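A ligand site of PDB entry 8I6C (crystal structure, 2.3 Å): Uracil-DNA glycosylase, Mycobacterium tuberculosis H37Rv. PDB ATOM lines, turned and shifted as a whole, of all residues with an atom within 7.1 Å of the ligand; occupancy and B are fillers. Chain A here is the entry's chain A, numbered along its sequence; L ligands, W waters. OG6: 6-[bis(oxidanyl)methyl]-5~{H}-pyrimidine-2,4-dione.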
ATOM      1  N   VAL A  76      -1.052  29.505  21.214  1.00  0.00           N
ATOM      2  CA  VAL A  76      -2.175  30.114  20.441  1.00  0.00           C
ATOM      3  C   VAL A  76      -1.628  30.539  19.087  1.00  0.00           C
ATOM      4  O   VAL A  76      -0.657  31.291  19.082  1.00  0.00           O
ATOM      5  CB  VAL A  76      -2.790  31.309  21.180  1.00  0.00           C
ATOM      6  CG1 VAL A  76      -4.035  31.803  20.463  1.00  0.00           C
ATOM      7  CG2 VAL A  76      -3.120  30.946  22.620  1.00  0.00           C
ATOM      8  N   GLY A  77      -2.293  30.124  18.008  1.00  0.00           N
ATOM      9  CA  GLY A  77      -2.076  30.617  16.637  1.00  0.00           C
ATOM     10  C   GLY A  77      -3.318  31.298  16.115  1.00  0.00           C
ATOM     11  O   GLY A  77      -4.268  31.495  16.887  1.00  0.00           O
ATOM     12  N   GLN A  78      -3.345  31.662  14.848  1.00  0.00           N
ATOM     13  CA  GLN A  78      -4.466  32.506  14.350  1.00  0.00           C
ATOM     14  C   GLN A  78      -5.373  31.600  13.495  1.00  0.00           C
ATOM     15  O   GLN A  78      -6.499  31.261  13.939  1.00  0.00           O
ATOM     16  CB  GLN A  78      -3.914  33.781  13.689  1.00  0.00           C
ATOM     17  CG  GLN A  78      -4.976  34.884  13.465  1.00  0.00           C
ATOM     18  CD  GLN A  78      -5.875  35.251  14.633  1.00  0.00           C
ATOM     19  OE1 GLN A  78      -7.106  35.143  14.566  1.00  0.00           O
ATOM     20  NE2 GLN A  78      -5.280  35.744  15.706  1.00  0.00           N
ATOM     21  N   ASP A  79      -4.856  31.178  12.359  1.00  0.00           N
ATOM     22  CA  ASP A  79      -5.594  30.390  11.346  1.00  0.00           C
ATOM     23  C   ASP A  79      -4.777  29.153  11.029  1.00  0.00           C
ATOM     24  O   ASP A  79      -3.552  29.205  11.151  1.00  0.00           O
ATOM     25  CB  ASP A  79      -5.805  31.200  10.066  1.00  0.00           C
ATOM     26  CG  ASP A  79      -6.504  32.518  10.315  1.00  0.00           C
ATOM     27  OD1 ASP A  79      -7.721  32.488  10.559  1.00  0.00           O
ATOM     28  OD2 ASP A  79      -5.803  33.574  10.261  1.00  0.00           O
ATOM     29  N   PRO A  80      -5.436  28.039  10.629  1.00  0.00           N
ATOM     30  CA  PRO A  80      -4.748  26.903  10.026  1.00  0.00           C
ATOM     31  C   PRO A  80      -3.905  27.218   8.766  1.00  0.00           C
ATOM     32  O   PRO A  80      -4.138  28.199   8.063  1.00  0.00           O
ATOM     33  CB  PRO A  80      -5.903  25.942   9.644  1.00  0.00           C
ATOM     34  CG  PRO A  80      -7.065  26.323  10.544  1.00  0.00           C
ATOM     35  CD  PRO A  80      -6.881  27.812  10.761  1.00  0.00           C
ATOM     36  N   TYR A  81      -2.968  26.323   8.478  1.00  0.00           N
ATOM     37  CA  TYR A  81      -2.213  26.305   7.212  1.00  0.00           C
ATOM     38  C   TYR A  81      -3.209  26.367   6.047  1.00  0.00           C
ATOM     39  O   TYR A  81      -4.169  25.606   5.989  1.00  0.00           O
ATOM     40  CB  TYR A  81      -1.356  25.032   7.139  1.00  0.00           C
ATOM     41  CG  TYR A  81      -0.200  24.963   8.118  1.00  0.00           C
ATOM     42  CD1 TYR A  81       0.836  25.889   8.085  1.00  0.00           C
ATOM     43  CD2 TYR A  81      -0.116  23.924   9.036  1.00  0.00           C
ATOM     44  CE1 TYR A  81       1.921  25.791   8.956  1.00  0.00           C
ATOM     45  CE2 TYR A  81       0.963  23.814   9.902  1.00  0.00           C
ATOM     46  CZ  TYR A  81       1.986  24.745   9.852  1.00  0.00           C
ATOM     47  OH  TYR A  81       3.043  24.645  10.721  1.00  0.00           O
ATOM     48  N   PRO A  82      -3.018  27.280   5.078  1.00  0.00           N
ATOM     49  CA  PRO A  82      -3.911  27.391   3.913  1.00  0.00           C
ATOM     50  C   PRO A  82      -3.592  26.418   2.771  1.00  0.00           C
ATOM     51  O   PRO A  82      -4.409  26.285   1.882  1.00  0.00           O
ATOM     52  CB  PRO A  82      -3.663  28.845   3.478  1.00  0.00           C
ATOM     53  CG  PRO A  82      -2.191  29.071   3.801  1.00  0.00           C
ATOM     54  CD  PRO A  82      -1.930  28.267   5.060  1.00  0.00           C
ATOM     55  N   ALA A  87      -2.830  21.479   7.261  1.00  0.00           N
ATOM     56  CA  ALA A  87      -3.673  21.646   8.482  1.00  0.00           C
ATOM     57  C   ALA A  87      -4.202  20.295   8.968  1.00  0.00           C
ATOM     58  O   ALA A  87      -4.849  19.567   8.159  1.00  0.00           O
ATOM     59  CB  ALA A  87      -4.799  22.601   8.202  1.00  0.00           C
ATOM     60  N   LEU A  90      -4.323  20.638  14.942  1.00  0.00           N
ATOM     61  CA  LEU A  90      -3.451  21.131  16.028  1.00  0.00           C
ATOM     62  C   LEU A  90      -2.609  22.261  15.449  1.00  0.00           C
ATOM     63  O   LEU A  90      -2.006  22.053  14.409  1.00  0.00           O
ATOM     64  CB  LEU A  90      -2.576  19.984  16.512  1.00  0.00           C
ATOM     65  CG  LEU A  90      -3.290  18.716  16.996  1.00  0.00           C
ATOM     66  CD1 LEU A  90      -2.257  17.690  17.402  1.00  0.00           C
ATOM     67  CD2 LEU A  90      -4.216  18.974  18.189  1.00  0.00           C
ATOM     68  N   SER A  91      -2.555  23.416  16.095  1.00  0.00           N
ATOM     69  CA  SER A  91      -1.862  24.622  15.555  1.00  0.00           C
ATOM     70  C   SER A  91      -0.410  24.253  15.231  1.00  0.00           C
ATOM     71  O   SER A  91       0.221  23.540  16.074  1.00  0.00           O
ATOM     72  CB  SER A  91      -1.944  25.753  16.518  1.00  0.00           C
ATOM     73  OG  SER A  91      -1.422  25.351  17.768  1.00  0.00           O
ATOM     74  N   PHE A  92       0.049  24.623  14.022  1.00  0.00           N
ATOM     75  CA  PHE A  92       1.455  24.499  13.521  1.00  0.00           C
ATOM     76  C   PHE A  92       1.871  23.078  13.135  1.00  0.00           C
ATOM     77  O   PHE A  92       2.836  22.962  12.346  1.00  0.00           O
ATOM     78  CB  PHE A  92       2.393  25.079  14.569  1.00  0.00           C
ATOM     79  CG  PHE A  92       2.103  26.532  14.799  1.00  0.00           C
ATOM     80  CD1 PHE A  92       2.400  27.461  13.826  1.00  0.00           C
ATOM     81  CD2 PHE A  92       1.471  26.954  15.956  1.00  0.00           C
ATOM     82  CE1 PHE A  92       2.113  28.808  14.022  1.00  0.00           C
ATOM     83  CE2 PHE A  92       1.206  28.296  16.163  1.00  0.00           C
ATOM     84  CZ  PHE A  92       1.530  29.227  15.191  1.00  0.00           C
ATOM     85  N   SER A  93       1.174  22.051  13.611  1.00  0.00           N
ATOM     86  CA  SER A  93       1.485  20.613  13.356  1.00  0.00           C
ATOM     87  C   SER A  93       1.186  20.310  11.898  1.00  0.00           C
ATOM     88  O   SER A  93       0.325  20.979  11.326  1.00  0.00           O
ATOM     89  CB  SER A  93       0.730  19.694  14.254  1.00  0.00           C
ATOM     90  OG  SER A  93       1.171  18.354  14.082  1.00  0.00           O
ATOM     91  N   PRO A 102       6.510  23.254   6.613  1.00  0.00           N
ATOM     92  CA  PRO A 102       6.288  24.684   6.395  1.00  0.00           C
ATOM     93  C   PRO A 102       7.272  25.585   7.153  1.00  0.00           C
ATOM     94  O   PRO A 102       7.696  25.184   8.224  1.00  0.00           O
ATOM     95  CB  PRO A 102       4.902  24.936   6.998  1.00  0.00           C
ATOM     96  CG  PRO A 102       4.284  23.568   7.148  1.00  0.00           C
ATOM     97  CD  PRO A 102       5.417  22.593   7.331  1.00  0.00           C
ATOM     98  N   SER A 104       7.019  28.168   9.083  1.00  0.00           N
ATOM     99  CA  SER A 104       6.577  28.355  10.491  1.00  0.00           C
ATOM    100  C   SER A 104       7.110  27.221  11.383  1.00  0.00           C
ATOM    101  O   SER A 104       7.708  27.511  12.445  1.00  0.00           O
ATOM    102  CB  SER A 104       5.074  28.455  10.569  1.00  0.00           C
ATOM    103  OG  SER A 104       4.626  29.767  10.221  1.00  0.00           O
ATOM    104  N   LEU A 105       6.912  25.968  10.950  1.00  0.00           N
ATOM    105  CA  LEU A 105       7.255  24.784  11.755  1.00  0.00           C
ATOM    106  C   LEU A 105       8.773  24.617  11.759  1.00  0.00           C
ATOM    107  O   LEU A 105       9.345  24.313  12.841  1.00  0.00           O
ATOM    108  CB  LEU A 105       6.505  23.571  11.193  1.00  0.00           C
ATOM    109  CG  LEU A 105       6.652  22.269  11.997  1.00  0.00           C
ATOM    110  CD1 LEU A 105       6.139  22.437  13.421  1.00  0.00           C
ATOM    111  CD2 LEU A 105       5.947  21.127  11.283  1.00  0.00           C
ATOM    112  N   LEU A 136      -2.564  23.106  21.450  1.00  0.00           N
ATOM    113  CA  LEU A 136      -2.197  23.773  20.200  1.00  0.00           C
ATOM    114  C   LEU A 136      -3.469  24.361  19.586  1.00  0.00           C
ATOM    115  O   LEU A 136      -4.034  23.762  18.638  1.00  0.00           O
ATOM    116  CB  LEU A 136      -1.501  22.727  19.317  1.00  0.00           C
ATOM    117  CG  LEU A 136      -0.261  22.087  19.938  1.00  0.00           C
ATOM    118  CD1 LEU A 136      -0.008  20.723  19.299  1.00  0.00           C
ATOM    119  CD2 LEU A 136       0.964  22.960  19.765  1.00  0.00           C
ATOM    120  N   LEU A 137      -3.918  25.488  20.113  1.00  0.00           N
ATOM    121  CA  LEU A 137      -5.207  26.065  19.701  1.00  0.00           C
ATOM    122  C   LEU A 137      -5.002  27.194  18.681  1.00  0.00           C
ATOM    123  O   LEU A 137      -4.374  28.208  19.005  1.00  0.00           O
ATOM    124  CB  LEU A 137      -5.941  26.550  20.942  1.00  0.00           C
ATOM    125  CG  LEU A 137      -7.334  27.109  20.662  1.00  0.00           C
ATOM    126  CD1 LEU A 137      -8.259  26.040  20.123  1.00  0.00           C
ATOM    127  CD2 LEU A 137      -7.957  27.733  21.890  1.00  0.00           C
ATOM    128  N   ASN A 138      -5.599  27.066  17.502  1.00  0.00           N
ATOM    129  CA  ASN A 138      -5.806  28.232  16.579  1.00  0.00           C
ATOM    130  C   ASN A 138      -7.067  29.007  16.984  1.00  0.00           C
ATOM    131  O   ASN A 138      -8.065  28.402  17.425  1.00  0.00           O
ATOM    132  CB  ASN A 138      -5.844  27.759  15.127  1.00  0.00           C
ATOM    133  CG  ASN A 138      -4.494  27.536  14.490  1.00  0.00           C
ATOM    134  OD1 ASN A 138      -3.519  28.232  14.770  1.00  0.00           O
ATOM    135  ND2 ASN A 138      -4.428  26.563  13.596  1.00  0.00           N
ATOM    136  N   ARG A 139      -7.072  30.339  16.843  1.00  0.00           N
ATOM    137  CA  ARG A 139      -8.238  31.173  17.251  1.00  0.00           C
ATOM    138  C   ARG A 139      -9.413  30.938  16.277  1.00  0.00           C
ATOM    139  O   ARG A 139     -10.571  31.125  16.695  1.00  0.00           O
ATOM    140  CB  ARG A 139      -7.916  32.675  17.252  1.00  0.00           C
ATOM    141  CG  ARG A 139      -7.152  33.184  18.473  1.00  0.00           C
ATOM    142  CD  ARG A 139      -7.855  33.020  19.815  1.00  0.00           C
ATOM    143  NE  ARG A 139      -9.281  33.379  19.937  1.00  0.00           N
ATOM    144  CZ  ARG A 139      -9.783  34.601  19.814  1.00  0.00           C
ATOM    145  NH1 ARG A 139     -11.086  34.798  19.995  1.00  0.00           N
ATOM    146  NH2 ARG A 139      -8.995  35.616  19.512  1.00  0.00           N
ATOM    147  N   VAL A 140      -9.075  30.626  15.026  1.00  0.00           N
ATOM    148  CA  VAL A 140      -9.999  30.276  13.907  1.00  0.00           C
ATOM    149  C   VAL A 140      -9.596  28.860  13.474  1.00  0.00           C
ATOM    150  O   VAL A 140      -8.392  28.637  13.196  1.00  0.00           O
ATOM    151  CB  VAL A 140      -9.940  31.335  12.793  1.00  0.00           C
ATOM    152  CG1 VAL A 140     -11.035  31.134  11.748  1.00  0.00           C
ATOM    153  CG2 VAL A 140     -10.008  32.760  13.323  1.00  0.00           C
ATOM    154  N   TRP A 179       1.698  32.748  19.667  1.00  0.00           N
ATOM    155  CA  TRP A 179       2.381  32.705  18.336  1.00  0.00           C
ATOM    156  C   TRP A 179       1.478  33.253  17.227  1.00  0.00           C
ATOM    157  O   TRP A 179       1.895  33.143  16.067  1.00  0.00           O
ATOM    158  CB  TRP A 179       2.864  31.293  17.997  1.00  0.00           C
ATOM    159  CG  TRP A 179       4.042  30.866  18.806  1.00  0.00           C
ATOM    160  CD1 TRP A 179       4.865  31.660  19.556  1.00  0.00           C
ATOM    161  CD2 TRP A 179       4.532  29.522  18.944  1.00  0.00           C
ATOM    162  NE1 TRP A 179       5.831  30.904  20.163  1.00  0.00           N
ATOM    163  CE2 TRP A 179       5.654  29.591  19.802  1.00  0.00           C
ATOM    164  CE3 TRP A 179       4.174  28.300  18.377  1.00  0.00           C
ATOM    165  CZ2 TRP A 179       6.415  28.461  20.131  1.00  0.00           C
ATOM    166  CZ3 TRP A 179       4.889  27.189  18.742  1.00  0.00           C
ATOM    167  CH2 TRP A 179       5.982  27.260  19.612  1.00  0.00           C
ATOM    168  N   GLY A 180       0.310  33.831  17.522  1.00  0.00           N
ATOM    169  CA  GLY A 180      -0.503  34.538  16.497  1.00  0.00           C
ATOM    170  C   GLY A 180      -0.763  35.996  16.839  1.00  0.00           C
ATOM    171  O   GLY A 180      -1.911  36.439  16.672  1.00  0.00           O
ATOM    172  N   PRO A 205       6.556  32.632  14.999  1.00  0.00           N
ATOM    173  CA  PRO A 205       7.562  31.861  14.291  1.00  0.00           C
ATOM    174  C   PRO A 205       8.243  32.558  13.107  1.00  0.00           C
ATOM    175  O   PRO A 205       9.438  32.391  13.042  1.00  0.00           O
ATOM    176  CB  PRO A 205       6.779  30.641  13.848  1.00  0.00           C
ATOM    177  CG  PRO A 205       5.844  30.386  15.015  1.00  0.00           C
ATOM    178  CD  PRO A 205       5.462  31.781  15.479  1.00  0.00           C
ATOM    179  N   LEU A 206       7.504  33.350  12.306  1.00  0.00           N
ATOM    180  CA  LEU A 206       8.029  34.054  11.108  1.00  0.00           C
ATOM    181  C   LEU A 206       8.774  35.361  11.470  1.00  0.00           C
ATOM    182  O   LEU A 206       9.385  35.966  10.540  1.00  0.00           O
ATOM    183  CB  LEU A 206       6.878  34.335  10.131  1.00  0.00           C
ATOM    184  CG  LEU A 206       6.180  33.110   9.555  1.00  0.00           C
ATOM    185  CD1 LEU A 206       5.144  33.498   8.530  1.00  0.00           C
ATOM    186  CD2 LEU A 206       7.176  32.143   8.930  1.00  0.00           C
HETATM  187  O2  OG6 L   1       0.825  30.174   9.071  1.00  0.00           O
HETATM  188  C10 OG6 L   1       0.927  29.076   9.599  1.00  0.00           C
HETATM  189  C06 OG6 L   1       0.159  28.909  10.849  1.00  0.00           C
HETATM  190  C07 OG6 L   1      -0.348  27.644  11.168  1.00  0.00           C
HETATM  191  C09 OG6 L   1      -1.181  27.491  12.274  1.00  0.00           C
HETATM  192  O02 OG6 L   1      -1.639  26.364  12.555  1.00  0.00           O
HETATM  193  N05 OG6 L   1      -1.461  28.590  13.009  1.00  0.00           N
HETATM  194  C08 OG6 L   1      -0.964  29.812  12.657  1.00  0.00           C
HETATM  195  O01 OG6 L   1      -1.227  30.827  13.323  1.00  0.00           O
HETATM  196  N04 OG6 L   1      -0.184  29.986  11.593  1.00  0.00           N
HETATM  197  O   HOH W   1      -2.245  30.521   8.848  1.00  0.00           O
HETATM  198  O   HOH W   2      -2.797  24.331  11.111  1.00  0.00           O
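OD1 of Asn 138 is in hydrogen-bond range of N05 of the ligand. The backbone NH of Gln 78 sits at hydrogen-bond distance from an oxygen (O01) of the ligand, 2.7 Å away. N of Phe 92 is in hydrogen-bond range of O02 of the ligand (2.8 Å). The backbone carbonyl oxygen (O) of Asp 79 lies within hydrogen-bond range of a nitrogen (N05) of the ligand.
N of Gln 78 sits at hydrogen-bond distance from OD1 of Asn 138 (3.4 Å). The backbone carbonyl oxygen (O) of Gln 78 is in hydrogen-bond range of the backbone NH (N) of Arg 139. N of Val 140 lies within hydrogen-bond range of O of Gln 78. The backbone NH (N) of Gly 77 is in hydrogen-bond range of the backbone carbonyl oxygen (O) of Leu 137 (3.0 Å). O of Gly 77 sits at hydrogen-bond distance from N of Arg 139 (3.0 Å). The side-chain hydroxyl (OG) of Ser 91 sits at hydrogen-bond distance from the backbone NH (N) of Leu 137, 3.4 Å away. The backbone carbonyl oxygen (O) of Leu 136 lies within hydrogen-bond range of the backbone NH (N) of Ser 91 (3.0 Å).
Residues that only touch the ligand: Gly 77 (3.4 Å), Ser 91 (3.5 Å), Tyr 81 (3.5 Å) and Ser 104 (3.8 Å). Hydrophobic or aromatic side chains within 4 Å of the ligand: Tyr 81 and Phe 92. Along chain A the residues within 4 Å of the ligand span positions 77 to 138.
Water W2 lies within hydrogen-bond range of an oxygen (O02) of the ligand (2.7 Å) and the backbone NH of Tyr 81 (3.3 Å). Water W1 lies within hydrogen-bond range of O of Asp 79 (3.0 Å), O of Pro 80 (3.1 Å) and O2 of the ligand (3.1 Å).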
